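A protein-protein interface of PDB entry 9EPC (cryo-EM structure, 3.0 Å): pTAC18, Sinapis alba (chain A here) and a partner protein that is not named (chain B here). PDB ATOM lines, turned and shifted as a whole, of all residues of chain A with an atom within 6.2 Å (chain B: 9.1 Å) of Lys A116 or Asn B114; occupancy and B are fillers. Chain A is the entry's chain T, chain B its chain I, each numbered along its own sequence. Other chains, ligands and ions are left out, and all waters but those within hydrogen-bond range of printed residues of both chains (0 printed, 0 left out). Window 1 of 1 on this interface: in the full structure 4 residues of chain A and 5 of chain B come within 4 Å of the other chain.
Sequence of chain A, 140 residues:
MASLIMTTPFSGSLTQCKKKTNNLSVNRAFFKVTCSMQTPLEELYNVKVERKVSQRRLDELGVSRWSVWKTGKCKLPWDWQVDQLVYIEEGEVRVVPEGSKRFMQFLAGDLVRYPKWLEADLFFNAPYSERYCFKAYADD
Among the printed residues, merely in contact across the chains: Lys A116 with Asn B114 (3.7 Å), Trp A117 with Asn B112 (3.2 Å) and Trp A117 with Gly B113 (3.96 Å).
The side-chain amide nitrogen of Asn A46 lies close to the side-chain amide nitrogen of Asn B111, at 3.4 Å.
Of the printed residues of chain B, Lys A116 touches Asn B114. Asn B114 touches just one residue of chain A: Lys A116 (3.7 Å). Of chain B, only Asn B112 and Gly B113 come within 4 Å of Trp A117. Of the printed residues of chain B, Asn A46 touches Asn B111. Printed residues of chain A within 4 Å of Gly B113: Trp A117 (3.96 Å). Printed residues of chain A within 4 Å of Asn B111: Asn A46. Printed residues of chain A within 4 Å of Asn B112: Trp A117. Phe B119 touches none of the printed residues of chain A. The nearest residue of chain B that does not touch Lys A116 is Gly B113 (6.3 Å). The nearest printed residue of chain A that does not touch Gly B113 is Tyr A137 (6.0 Å).
The backbone NH (N) of Trp A117 sits at hydrogen-bond distance from the backbone carbonyl oxygen (O) of Trp A80, 2.6 Å away. The backbone carbonyl oxygen (O) of Asn B114 lies close to the side-chain amide nitrogen (ND2) of Asn B111, at 3.4 Å.
Of the 16 printed residues of chain B, 4 touch a printed residue of chain A. Printed residues of chain A that touch a printed residue of chain B: Asn A46, Lys A116 and Trp A117. Hydrophobic or aromatic side chains of chain A within 4 Å of the printed part of chain B: Trp A117. Among the printed residues, 4 pairs touch across the chains. Among the printed residues, no Asp or Glu carboxylate lies within 4 Å of a Lys or Arg side-chain nitrogen of the other chain.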
ATOM      1  N   ASN A  46      19.560   9.856   4.752  1.00  0.00           N
ATOM      2  CA  ASN A  46      19.317   9.979   3.313  1.00  0.00           C
ATOM      3  C   ASN A  46      20.615   9.884   2.514  1.00  0.00           C
ATOM      4  O   ASN A  46      20.907  10.702   1.640  1.00  0.00           O
ATOM      5  CB  ASN A  46      18.545  11.262   2.984  1.00  0.00           C
ATOM      6  CG  ASN A  46      19.308  12.526   3.333  1.00  0.00           C
ATOM      7  OD1 ASN A  46      19.221  13.029   4.453  1.00  0.00           O
ATOM      8  ND2 ASN A  46      20.054  13.051   2.368  1.00  0.00           N
ATOM      9  N   TRP A  80      30.318  17.193   5.594  1.00  0.00           N
ATOM     10  CA  TRP A  80      30.119  17.510   4.183  1.00  0.00           C
ATOM     11  C   TRP A  80      29.447  18.869   4.062  1.00  0.00           C
ATOM     12  O   TRP A  80      28.237  19.000   4.254  1.00  0.00           O
ATOM     13  CB  TRP A  80      29.296  16.423   3.503  1.00  0.00           C
ATOM     14  CG  TRP A  80      30.086  15.194   3.202  1.00  0.00           C
ATOM     15  CD1 TRP A  80      30.668  14.869   2.015  1.00  0.00           C
ATOM     16  CD2 TRP A  80      30.391  14.128   4.105  1.00  0.00           C
ATOM     17  NE1 TRP A  80      31.314  13.663   2.120  1.00  0.00           N
ATOM     18  CE2 TRP A  80      31.160  13.187   3.395  1.00  0.00           C
ATOM     19  CE3 TRP A  80      30.088  13.875   5.444  1.00  0.00           C
ATOM     20  CZ2 TRP A  80      31.628  12.016   3.979  1.00  0.00           C
ATOM     21  CZ3 TRP A  80      30.553  12.712   6.021  1.00  0.00           C
ATOM     22  CH2 TRP A  80      31.314  11.796   5.290  1.00  0.00           C
ATOM     23  N   GLN A  81      30.240  19.892   3.739  1.00  0.00           N
ATOM     24  CA  GLN A  81      29.693  21.207   3.431  1.00  0.00           C
ATOM     25  C   GLN A  81      29.049  21.259   2.055  1.00  0.00           C
ATOM     26  O   GLN A  81      28.409  22.263   1.728  1.00  0.00           O
ATOM     27  CB  GLN A  81      30.790  22.269   3.525  1.00  0.00           C
ATOM     28  CG  GLN A  81      31.287  22.532   4.935  1.00  0.00           C
ATOM     29  CD  GLN A  81      32.610  23.269   4.951  1.00  0.00           C
ATOM     30  OE1 GLN A  81      33.192  23.543   3.902  1.00  0.00           O
ATOM     31  NE2 GLN A  81      33.095  23.590   6.144  1.00  0.00           N
ATOM     32  N   VAL A  82      29.213  20.216   1.244  1.00  0.00           N
ATOM     33  CA  VAL A  82      28.596  20.142  -0.073  1.00  0.00           C
ATOM     34  C   VAL A  82      28.362  18.673  -0.395  1.00  0.00           C
ATOM     35  O   VAL A  82      29.053  17.790   0.121  1.00  0.00           O
ATOM     36  CB  VAL A  82      29.467  20.833  -1.152  1.00  0.00           C
ATOM     37  CG1 VAL A  82      30.704  20.009  -1.449  1.00  0.00           C
ATOM     38  CG2 VAL A  82      28.662  21.088  -2.417  1.00  0.00           C
ATOM     39  N   ASP A  83      27.363  18.413  -1.234  1.00  0.00           N
ATOM     40  CA  ASP A  83      27.030  17.044  -1.599  1.00  0.00           C
ATOM     41  C   ASP A  83      28.210  16.380  -2.298  1.00  0.00           C
ATOM     42  O   ASP A  83      28.861  16.976  -3.160  1.00  0.00           O
ATOM     43  CB  ASP A  83      25.799  17.026  -2.506  1.00  0.00           C
ATOM     44  CG  ASP A  83      25.209  15.638  -2.672  1.00  0.00           C
ATOM     45  OD1 ASP A  83      25.907  14.645  -2.376  1.00  0.00           O
ATOM     46  OD2 ASP A  83      24.042  15.537  -3.104  1.00  0.00           O
ATOM     47  N   GLN A  84      28.486  15.135  -1.917  1.00  0.00           N
ATOM     48  CA  GLN A  84      29.603  14.375  -2.462  1.00  0.00           C
ATOM     49  C   GLN A  84      29.101  13.037  -2.976  1.00  0.00           C
ATOM     50  O   GLN A  84      28.370  12.333  -2.272  1.00  0.00           O
ATOM     51  CB  GLN A  84      30.690  14.158  -1.410  1.00  0.00           C
ATOM     52  CG  GLN A  84      31.915  13.441  -1.939  1.00  0.00           C
ATOM     53  CD  GLN A  84      32.939  13.166  -0.858  1.00  0.00           C
ATOM     54  OE1 GLN A  84      32.628  13.203   0.330  1.00  0.00           O
ATOM     55  NE2 GLN A  84      34.171  12.888  -1.267  1.00  0.00           N
ATOM     56  N   TYR A 114      27.063  11.040  -0.100  1.00  0.00           N
ATOM     57  CA  TYR A 114      26.949  11.677   1.202  1.00  0.00           C
ATOM     58  C   TYR A 114      26.267  13.028   1.049  1.00  0.00           C
ATOM     59  O   TYR A 114      26.756  13.875   0.290  1.00  0.00           O
ATOM     60  CB  TYR A 114      28.323  11.851   1.834  1.00  0.00           C
ATOM     61  CG  TYR A 114      29.110  10.571   1.977  1.00  0.00           C
ATOM     62  CD1 TYR A 114      29.948  10.131   0.962  1.00  0.00           C
ATOM     63  CD2 TYR A 114      29.025   9.809   3.132  1.00  0.00           C
ATOM     64  CE1 TYR A 114      30.675   8.967   1.093  1.00  0.00           C
ATOM     65  CE2 TYR A 114      29.747   8.643   3.270  1.00  0.00           C
ATOM     66  CZ  TYR A 114      30.570   8.226   2.249  1.00  0.00           C
ATOM     67  OH  TYR A 114      31.290   7.063   2.384  1.00  0.00           O
ATOM     68  N   PRO A 115      25.159  13.278   1.733  1.00  0.00           N
ATOM     69  CA  PRO A 115      24.471  14.564   1.599  1.00  0.00           C
ATOM     70  C   PRO A 115      25.215  15.670   2.336  1.00  0.00           C
ATOM     71  O   PRO A 115      26.199  15.442   3.039  1.00  0.00           O
ATOM     72  CB  PRO A 115      23.106  14.297   2.234  1.00  0.00           C
ATOM     73  CG  PRO A 115      23.385  13.245   3.248  1.00  0.00           C
ATOM     74  CD  PRO A 115      24.457  12.370   2.654  1.00  0.00           C
ATOM     75  N   LYS A 116      24.716  16.888   2.160  1.00  0.00           N
ATOM     76  CA  LYS A 116      25.302  18.037   2.828  1.00  0.00           C
ATOM     77  C   LYS A 116      25.015  17.994   4.324  1.00  0.00           C
ATOM     78  O   LYS A 116      24.114  17.296   4.795  1.00  0.00           O
ATOM     79  CB  LYS A 116      24.761  19.339   2.242  1.00  0.00           C
ATOM     80  CG  LYS A 116      25.091  19.552   0.781  1.00  0.00           C
ATOM     81  CD  LYS A 116      24.696  20.947   0.335  1.00  0.00           C
ATOM     82  CE  LYS A 116      25.283  21.999   1.259  1.00  0.00           C
ATOM     83  NZ  LYS A 116      25.017  23.380   0.782  1.00  0.00           N
ATOM     84  N   TRP A 117      25.813  18.753   5.075  1.00  0.00           N
ATOM     85  CA  TRP A 117      25.617  18.961   6.507  1.00  0.00           C
ATOM     86  C   TRP A 117      25.654  17.658   7.296  1.00  0.00           C
ATOM     87  O   TRP A 117      25.063  17.566   8.375  1.00  0.00           O
ATOM     88  CB  TRP A 117      24.304  19.703   6.776  1.00  0.00           C
ATOM     89  CG  TRP A 117      24.136  20.921   5.929  1.00  0.00           C
ATOM     90  CD1 TRP A 117      25.116  21.774   5.519  1.00  0.00           C
ATOM     91  CD2 TRP A 117      22.916  21.412   5.370  1.00  0.00           C
ATOM     92  NE1 TRP A 117      24.580  22.774   4.746  1.00  0.00           N
ATOM     93  CE2 TRP A 117      23.229  22.573   4.639  1.00  0.00           C
ATOM     94  CE3 TRP A 117      21.586  20.986   5.419  1.00  0.00           C
ATOM     95  CZ2 TRP A 117      22.264  23.312   3.963  1.00  0.00           C
ATOM     96  CZ3 TRP A 117      20.629  21.720   4.748  1.00  0.00           C
ATOM     97  CH2 TRP A 117      20.973  22.870   4.030  1.00  0.00           C
ATOM     98  N   LEU A 118      26.338  16.644   6.775  1.00  0.00           N
ATOM     99  CA  LEU A 118      26.466  15.363   7.454  1.00  0.00           C
ATOM    100  C   LEU A 118      27.758  15.348   8.258  1.00  0.00           C
ATOM    101  O   LEU A 118      28.847  15.486   7.695  1.00  0.00           O
ATOM    102  CB  LEU A 118      26.451  14.215   6.447  1.00  0.00           C
ATOM    103  CG  LEU A 118      26.915  12.855   6.970  1.00  0.00           C
ATOM    104  CD1 LEU A 118      26.008  12.364   8.082  1.00  0.00           C
ATOM    105  CD2 LEU A 118      26.976  11.841   5.841  1.00  0.00           C
ATOM    106  N   LYS A 135      29.231  17.648  -5.761  1.00  0.00           N
ATOM    107  CA  LYS A 135      28.172  18.225  -6.578  1.00  0.00           C
ATOM    108  C   LYS A 135      27.493  19.348  -5.809  1.00  0.00           C
ATOM    109  O   LYS A 135      27.138  19.177  -4.639  1.00  0.00           O
ATOM    110  CB  LYS A 135      27.149  17.160  -6.977  1.00  0.00           C
ATOM    111  CG  LYS A 135      27.774  15.878  -7.500  1.00  0.00           C
ATOM    112  CD  LYS A 135      28.654  16.146  -8.710  1.00  0.00           C
ATOM    113  CE  LYS A 135      27.825  16.342  -9.964  1.00  0.00           C
ATOM    114  NZ  LYS A 135      27.113  15.089 -10.333  1.00  0.00           N
ATOM    115  N   TYR A 137      24.330  22.456  -5.751  1.00  0.00           N
ATOM    116  CA  TYR A 137      22.890  22.379  -5.948  1.00  0.00           C
ATOM    117  C   TYR A 137      22.574  22.253  -7.431  1.00  0.00           C
ATOM    118  O   TYR A 137      23.084  23.021  -8.252  1.00  0.00           O
ATOM    119  CB  TYR A 137      22.199  23.610  -5.367  1.00  0.00           C
ATOM    120  CG  TYR A 137      20.743  23.710  -5.754  1.00  0.00           C
ATOM    121  CD1 TYR A 137      19.772  23.004  -5.061  1.00  0.00           C
ATOM    122  CD2 TYR A 137      20.339  24.508  -6.816  1.00  0.00           C
ATOM    123  CE1 TYR A 137      18.440  23.089  -5.412  1.00  0.00           C
ATOM    124  CE2 TYR A 137      19.013  24.596  -7.175  1.00  0.00           C
ATOM    125  CZ  TYR A 137      18.067  23.888  -6.470  1.00  0.00           C
ATOM    126  OH  TYR A 137      16.741  23.976  -6.826  1.00  0.00           O
ATOM    127  N   ILE B 106       6.246  16.891  -0.459  1.00  0.00           N
ATOM    128  CA  ILE B 106       7.021  18.099  -0.727  1.00  0.00           C
ATOM    129  C   ILE B 106       7.991  18.370   0.414  1.00  0.00           C
ATOM    130  O   ILE B 106       9.174  18.654   0.194  1.00  0.00           O
ATOM    131  CB  ILE B 106       6.082  19.294  -0.961  1.00  0.00           C
ATOM    132  CG1 ILE B 106       5.230  19.057  -2.204  1.00  0.00           C
ATOM    133  CG2 ILE B 106       6.879  20.577  -1.089  1.00  0.00           C
ATOM    134  CD1 ILE B 106       4.264  20.169  -2.481  1.00  0.00           C
ATOM    135  N   LYS B 107       7.504  18.284   1.653  1.00  0.00           N
ATOM    136  CA  LYS B 107       8.361  18.554   2.800  1.00  0.00           C
ATOM    137  C   LYS B 107       9.476  17.524   2.915  1.00  0.00           C
ATOM    138  O   LYS B 107      10.620  17.874   3.225  1.00  0.00           O
ATOM    139  CB  LYS B 107       7.527  18.594   4.078  1.00  0.00           C
ATOM    140  CG  LYS B 107       8.264  19.159   5.277  1.00  0.00           C
ATOM    141  CD  LYS B 107       7.344  19.280   6.479  1.00  0.00           C
ATOM    142  CE  LYS B 107       8.060  19.919   7.655  1.00  0.00           C
ATOM    143  NZ  LYS B 107       9.257  19.138   8.065  1.00  0.00           N
ATOM    144  N   ALA B 108       9.164  16.250   2.672  1.00  0.00           N
ATOM    145  CA  ALA B 108      10.191  15.215   2.737  1.00  0.00           C
ATOM    146  C   ALA B 108      11.223  15.393   1.632  1.00  0.00           C
ATOM    147  O   ALA B 108      12.432  15.307   1.878  1.00  0.00           O
ATOM    148  CB  ALA B 108       9.548  13.830   2.654  1.00  0.00           C
ATOM    149  N   THR B 109      10.767  15.649   0.405  1.00  0.00           N
ATOM    150  CA  THR B 109      11.700  15.844  -0.700  1.00  0.00           C
ATOM    151  C   THR B 109      12.485  17.138  -0.550  1.00  0.00           C
ATOM    152  O   THR B 109      13.596  17.250  -1.078  1.00  0.00           O
ATOM    153  CB  THR B 109      10.954  15.831  -2.032  1.00  0.00           C
ATOM    154  OG1 THR B 109       9.818  16.699  -1.951  1.00  0.00           O
ATOM    155  CG2 THR B 109      10.494  14.426  -2.368  1.00  0.00           C
ATOM    156  N   TYR B 110      11.927  18.123   0.158  1.00  0.00           N
ATOM    157  CA  TYR B 110      12.667  19.350   0.423  1.00  0.00           C
ATOM    158  C   TYR B 110      13.925  19.070   1.233  1.00  0.00           C
ATOM    159  O   TYR B 110      14.947  19.739   1.045  1.00  0.00           O
ATOM    160  CB  TYR B 110      11.768  20.350   1.146  1.00  0.00           C
ATOM    161  CG  TYR B 110      12.437  21.659   1.488  1.00  0.00           C
ATOM    162  CD1 TYR B 110      12.827  22.542   0.494  1.00  0.00           C
ATOM    163  CD2 TYR B 110      12.661  22.019   2.809  1.00  0.00           C
ATOM    164  CE1 TYR B 110      13.432  23.742   0.804  1.00  0.00           C
ATOM    165  CE2 TYR B 110      13.260  23.218   3.129  1.00  0.00           C
ATOM    166  CZ  TYR B 110      13.646  24.074   2.123  1.00  0.00           C
ATOM    167  OH  TYR B 110      14.249  25.269   2.439  1.00  0.00           O
ATOM    168  N   ASN B 111      13.864  18.088   2.133  1.00  0.00           N
ATOM    169  CA  ASN B 111      15.025  17.621   2.890  1.00  0.00           C
ATOM    170  C   ASN B 111      15.682  18.760   3.664  1.00  0.00           C
ATOM    171  O   ASN B 111      16.908  18.845   3.764  1.00  0.00           O
ATOM    172  CB  ASN B 111      16.032  16.926   1.971  1.00  0.00           C
ATOM    173  CG  ASN B 111      17.034  16.090   2.736  1.00  0.00           C
ATOM    174  OD1 ASN B 111      16.791  15.697   3.875  1.00  0.00           O
ATOM    175  ND2 ASN B 111      18.171  15.813   2.111  1.00  0.00           N
ATOM    176  N   ASN B 112      14.852  19.646   4.216  1.00  0.00           N
ATOM    177  CA  ASN B 112      15.309  20.732   5.081  1.00  0.00           C
ATOM    178  C   ASN B 112      16.366  21.594   4.394  1.00  0.00           C
ATOM    179  O   ASN B 112      17.406  21.914   4.973  1.00  0.00           O
ATOM    180  CB  ASN B 112      15.829  20.188   6.412  1.00  0.00           C
ATOM    181  CG  ASN B 112      15.921  21.255   7.482  1.00  0.00           C
ATOM    182  OD1 ASN B 112      15.241  22.277   7.412  1.00  0.00           O
ATOM    183  ND2 ASN B 112      16.765  21.023   8.479  1.00  0.00           N
ATOM    184  N   GLY B 113      16.105  21.968   3.145  1.00  0.00           N
ATOM    185  CA  GLY B 113      16.962  22.883   2.424  1.00  0.00           C
ATOM    186  C   GLY B 113      17.916  22.248   1.439  1.00  0.00           C
ATOM    187  O   GLY B 113      18.684  22.972   0.796  1.00  0.00           O
ATOM    188  N   ASN B 114      17.894  20.927   1.294  1.00  0.00           N
ATOM    189  CA  ASN B 114      18.733  20.215   0.332  1.00  0.00           C
ATOM    190  C   ASN B 114      17.829  19.326  -0.510  1.00  0.00           C
ATOM    191  O   ASN B 114      17.791  18.103  -0.331  1.00  0.00           O
ATOM    192  CB  ASN B 114      19.817  19.401   1.039  1.00  0.00           C
ATOM    193  CG  ASN B 114      20.778  18.747   0.070  1.00  0.00           C
ATOM    194  OD1 ASN B 114      20.847  19.120  -1.101  1.00  0.00           O
ATOM    195  ND2 ASN B 114      21.528  17.765   0.554  1.00  0.00           N
ATOM    196  N   PRO B 115      17.086  19.918  -1.444  1.00  0.00           N
ATOM    197  CA  PRO B 115      16.016  19.178  -2.121  1.00  0.00           C
ATOM    198  C   PRO B 115      16.529  17.947  -2.855  1.00  0.00           C
ATOM    199  O   PRO B 115      17.606  17.955  -3.454  1.00  0.00           O
ATOM    200  CB  PRO B 115      15.439  20.208  -3.097  1.00  0.00           C
ATOM    201  CG  PRO B 115      15.817  21.531  -2.521  1.00  0.00           C
ATOM    202  CD  PRO B 115      17.154  21.320  -1.885  1.00  0.00           C
ATOM    203  N   LEU B 116      15.737  16.881  -2.791  1.00  0.00           N
ATOM    204  CA  LEU B 116      16.020  15.671  -3.533  1.00  0.00           C
ATOM    205  C   LEU B 116      15.721  15.892  -5.014  1.00  0.00           C
ATOM    206  O   LEU B 116      15.036  16.850  -5.379  1.00  0.00           O
ATOM    207  CB  LEU B 116      15.188  14.515  -2.983  1.00  0.00           C
ATOM    208  CG  LEU B 116      15.309  14.274  -1.478  1.00  0.00           C
ATOM    209  CD1 LEU B 116      14.504  13.057  -1.064  1.00  0.00           C
ATOM    210  CD2 LEU B 116      16.765  14.123  -1.076  1.00  0.00           C
ATOM    211  N   PRO B 117      16.239  15.028  -5.892  1.00  0.00           N
ATOM    212  CA  PRO B 117      15.954  15.200  -7.326  1.00  0.00           C
ATOM    213  C   PRO B 117      14.474  15.165  -7.656  1.00  0.00           C
ATOM    214  O   PRO B 117      14.061  15.745  -8.668  1.00  0.00           O
ATOM    215  CB  PRO B 117      16.703  14.027  -7.972  1.00  0.00           C
ATOM    216  CG  PRO B 117      17.796  13.715  -7.017  1.00  0.00           C
ATOM    217  CD  PRO B 117      17.224  13.958  -5.654  1.00  0.00           C
ATOM    218  N   GLU B 118      13.662  14.505  -6.834  1.00  0.00           N
ATOM    219  CA  GLU B 118      12.227  14.447  -7.069  1.00  0.00           C
ATOM    220  C   GLU B 118      11.491  15.680  -6.565  1.00  0.00           C
ATOM    221  O   GLU B 118      10.299  15.825  -6.850  1.00  0.00           O
ATOM    222  CB  GLU B 118      11.634  13.201  -6.406  1.00  0.00           C
ATOM    223  CG  GLU B 118      12.301  11.891  -6.802  1.00  0.00           C
ATOM    224  CD  GLU B 118      13.555  11.591  -5.997  1.00  0.00           C
ATOM    225  OE1 GLU B 118      14.100  12.520  -5.365  1.00  0.00           O
ATOM    226  OE2 GLU B 118      13.994  10.422  -5.997  1.00  0.00           O
ATOM    227  N   PHE B 119      12.166  16.563  -5.825  1.00  0.00           N
ATOM    228  CA  PHE B 119      11.479  17.706  -5.232  1.00  0.00           C
ATOM    229  C   PHE B 119      10.941  18.657  -6.293  1.00  0.00           C
ATOM    230  O   PHE B 119       9.814  19.148  -6.175  1.00  0.00           O
ATOM    231  CB  PHE B 119      12.413  18.450  -4.282  1.00  0.00           C
ATOM    232  CG  PHE B 119      11.846  19.741  -3.768  1.00  0.00           C
ATOM    233  CD1 PHE B 119      10.949  19.745  -2.715  1.00  0.00           C
ATOM    234  CD2 PHE B 119      12.207  20.948  -4.337  1.00  0.00           C
ATOM    235  CE1 PHE B 119      10.424  20.928  -2.241  1.00  0.00           C
ATOM    236  CE2 PHE B 119      11.683  22.134  -3.868  1.00  0.00           C
ATOM    237  CZ  PHE B 119      10.791  22.124  -2.818  1.00  0.00           C
ATOM    238  N   ILE B 198      10.006  26.328  -5.069  1.00  0.00           N
ATOM    239  CA  ILE B 198       9.859  26.420  -3.622  1.00  0.00           C
ATOM    240  C   ILE B 198       8.459  26.904  -3.281  1.00  0.00           C
ATOM    241  O   ILE B 198       7.946  27.856  -3.881  1.00  0.00           O
ATOM    242  CB  ILE B 198      10.931  27.348  -3.034  1.00  0.00           C
ATOM    243  CG1 ILE B 198      12.328  26.845  -3.397  1.00  0.00           C
ATOM    244  CG2 ILE B 198      10.784  27.445  -1.526  1.00  0.00           C
ATOM    245  CD1 ILE B 198      12.633  25.467  -2.864  1.00  0.00           C
ATOM    246  N   VAL B 202       7.156  23.774   2.678  1.00  0.00           N
ATOM    247  CA  VAL B 202       8.422  23.345   3.252  1.00  0.00           C
ATOM    248  C   VAL B 202       8.653  23.951   4.629  1.00  0.00           C
ATOM    249  O   VAL B 202       9.459  23.425   5.404  1.00  0.00           O
ATOM    250  CB  VAL B 202       9.578  23.691   2.296  1.00  0.00           C
ATOM    251  CG1 VAL B 202       9.291  23.142   0.912  1.00  0.00           C
ATOM    252  CG2 VAL B 202       9.795  25.188   2.243  1.00  0.00           C
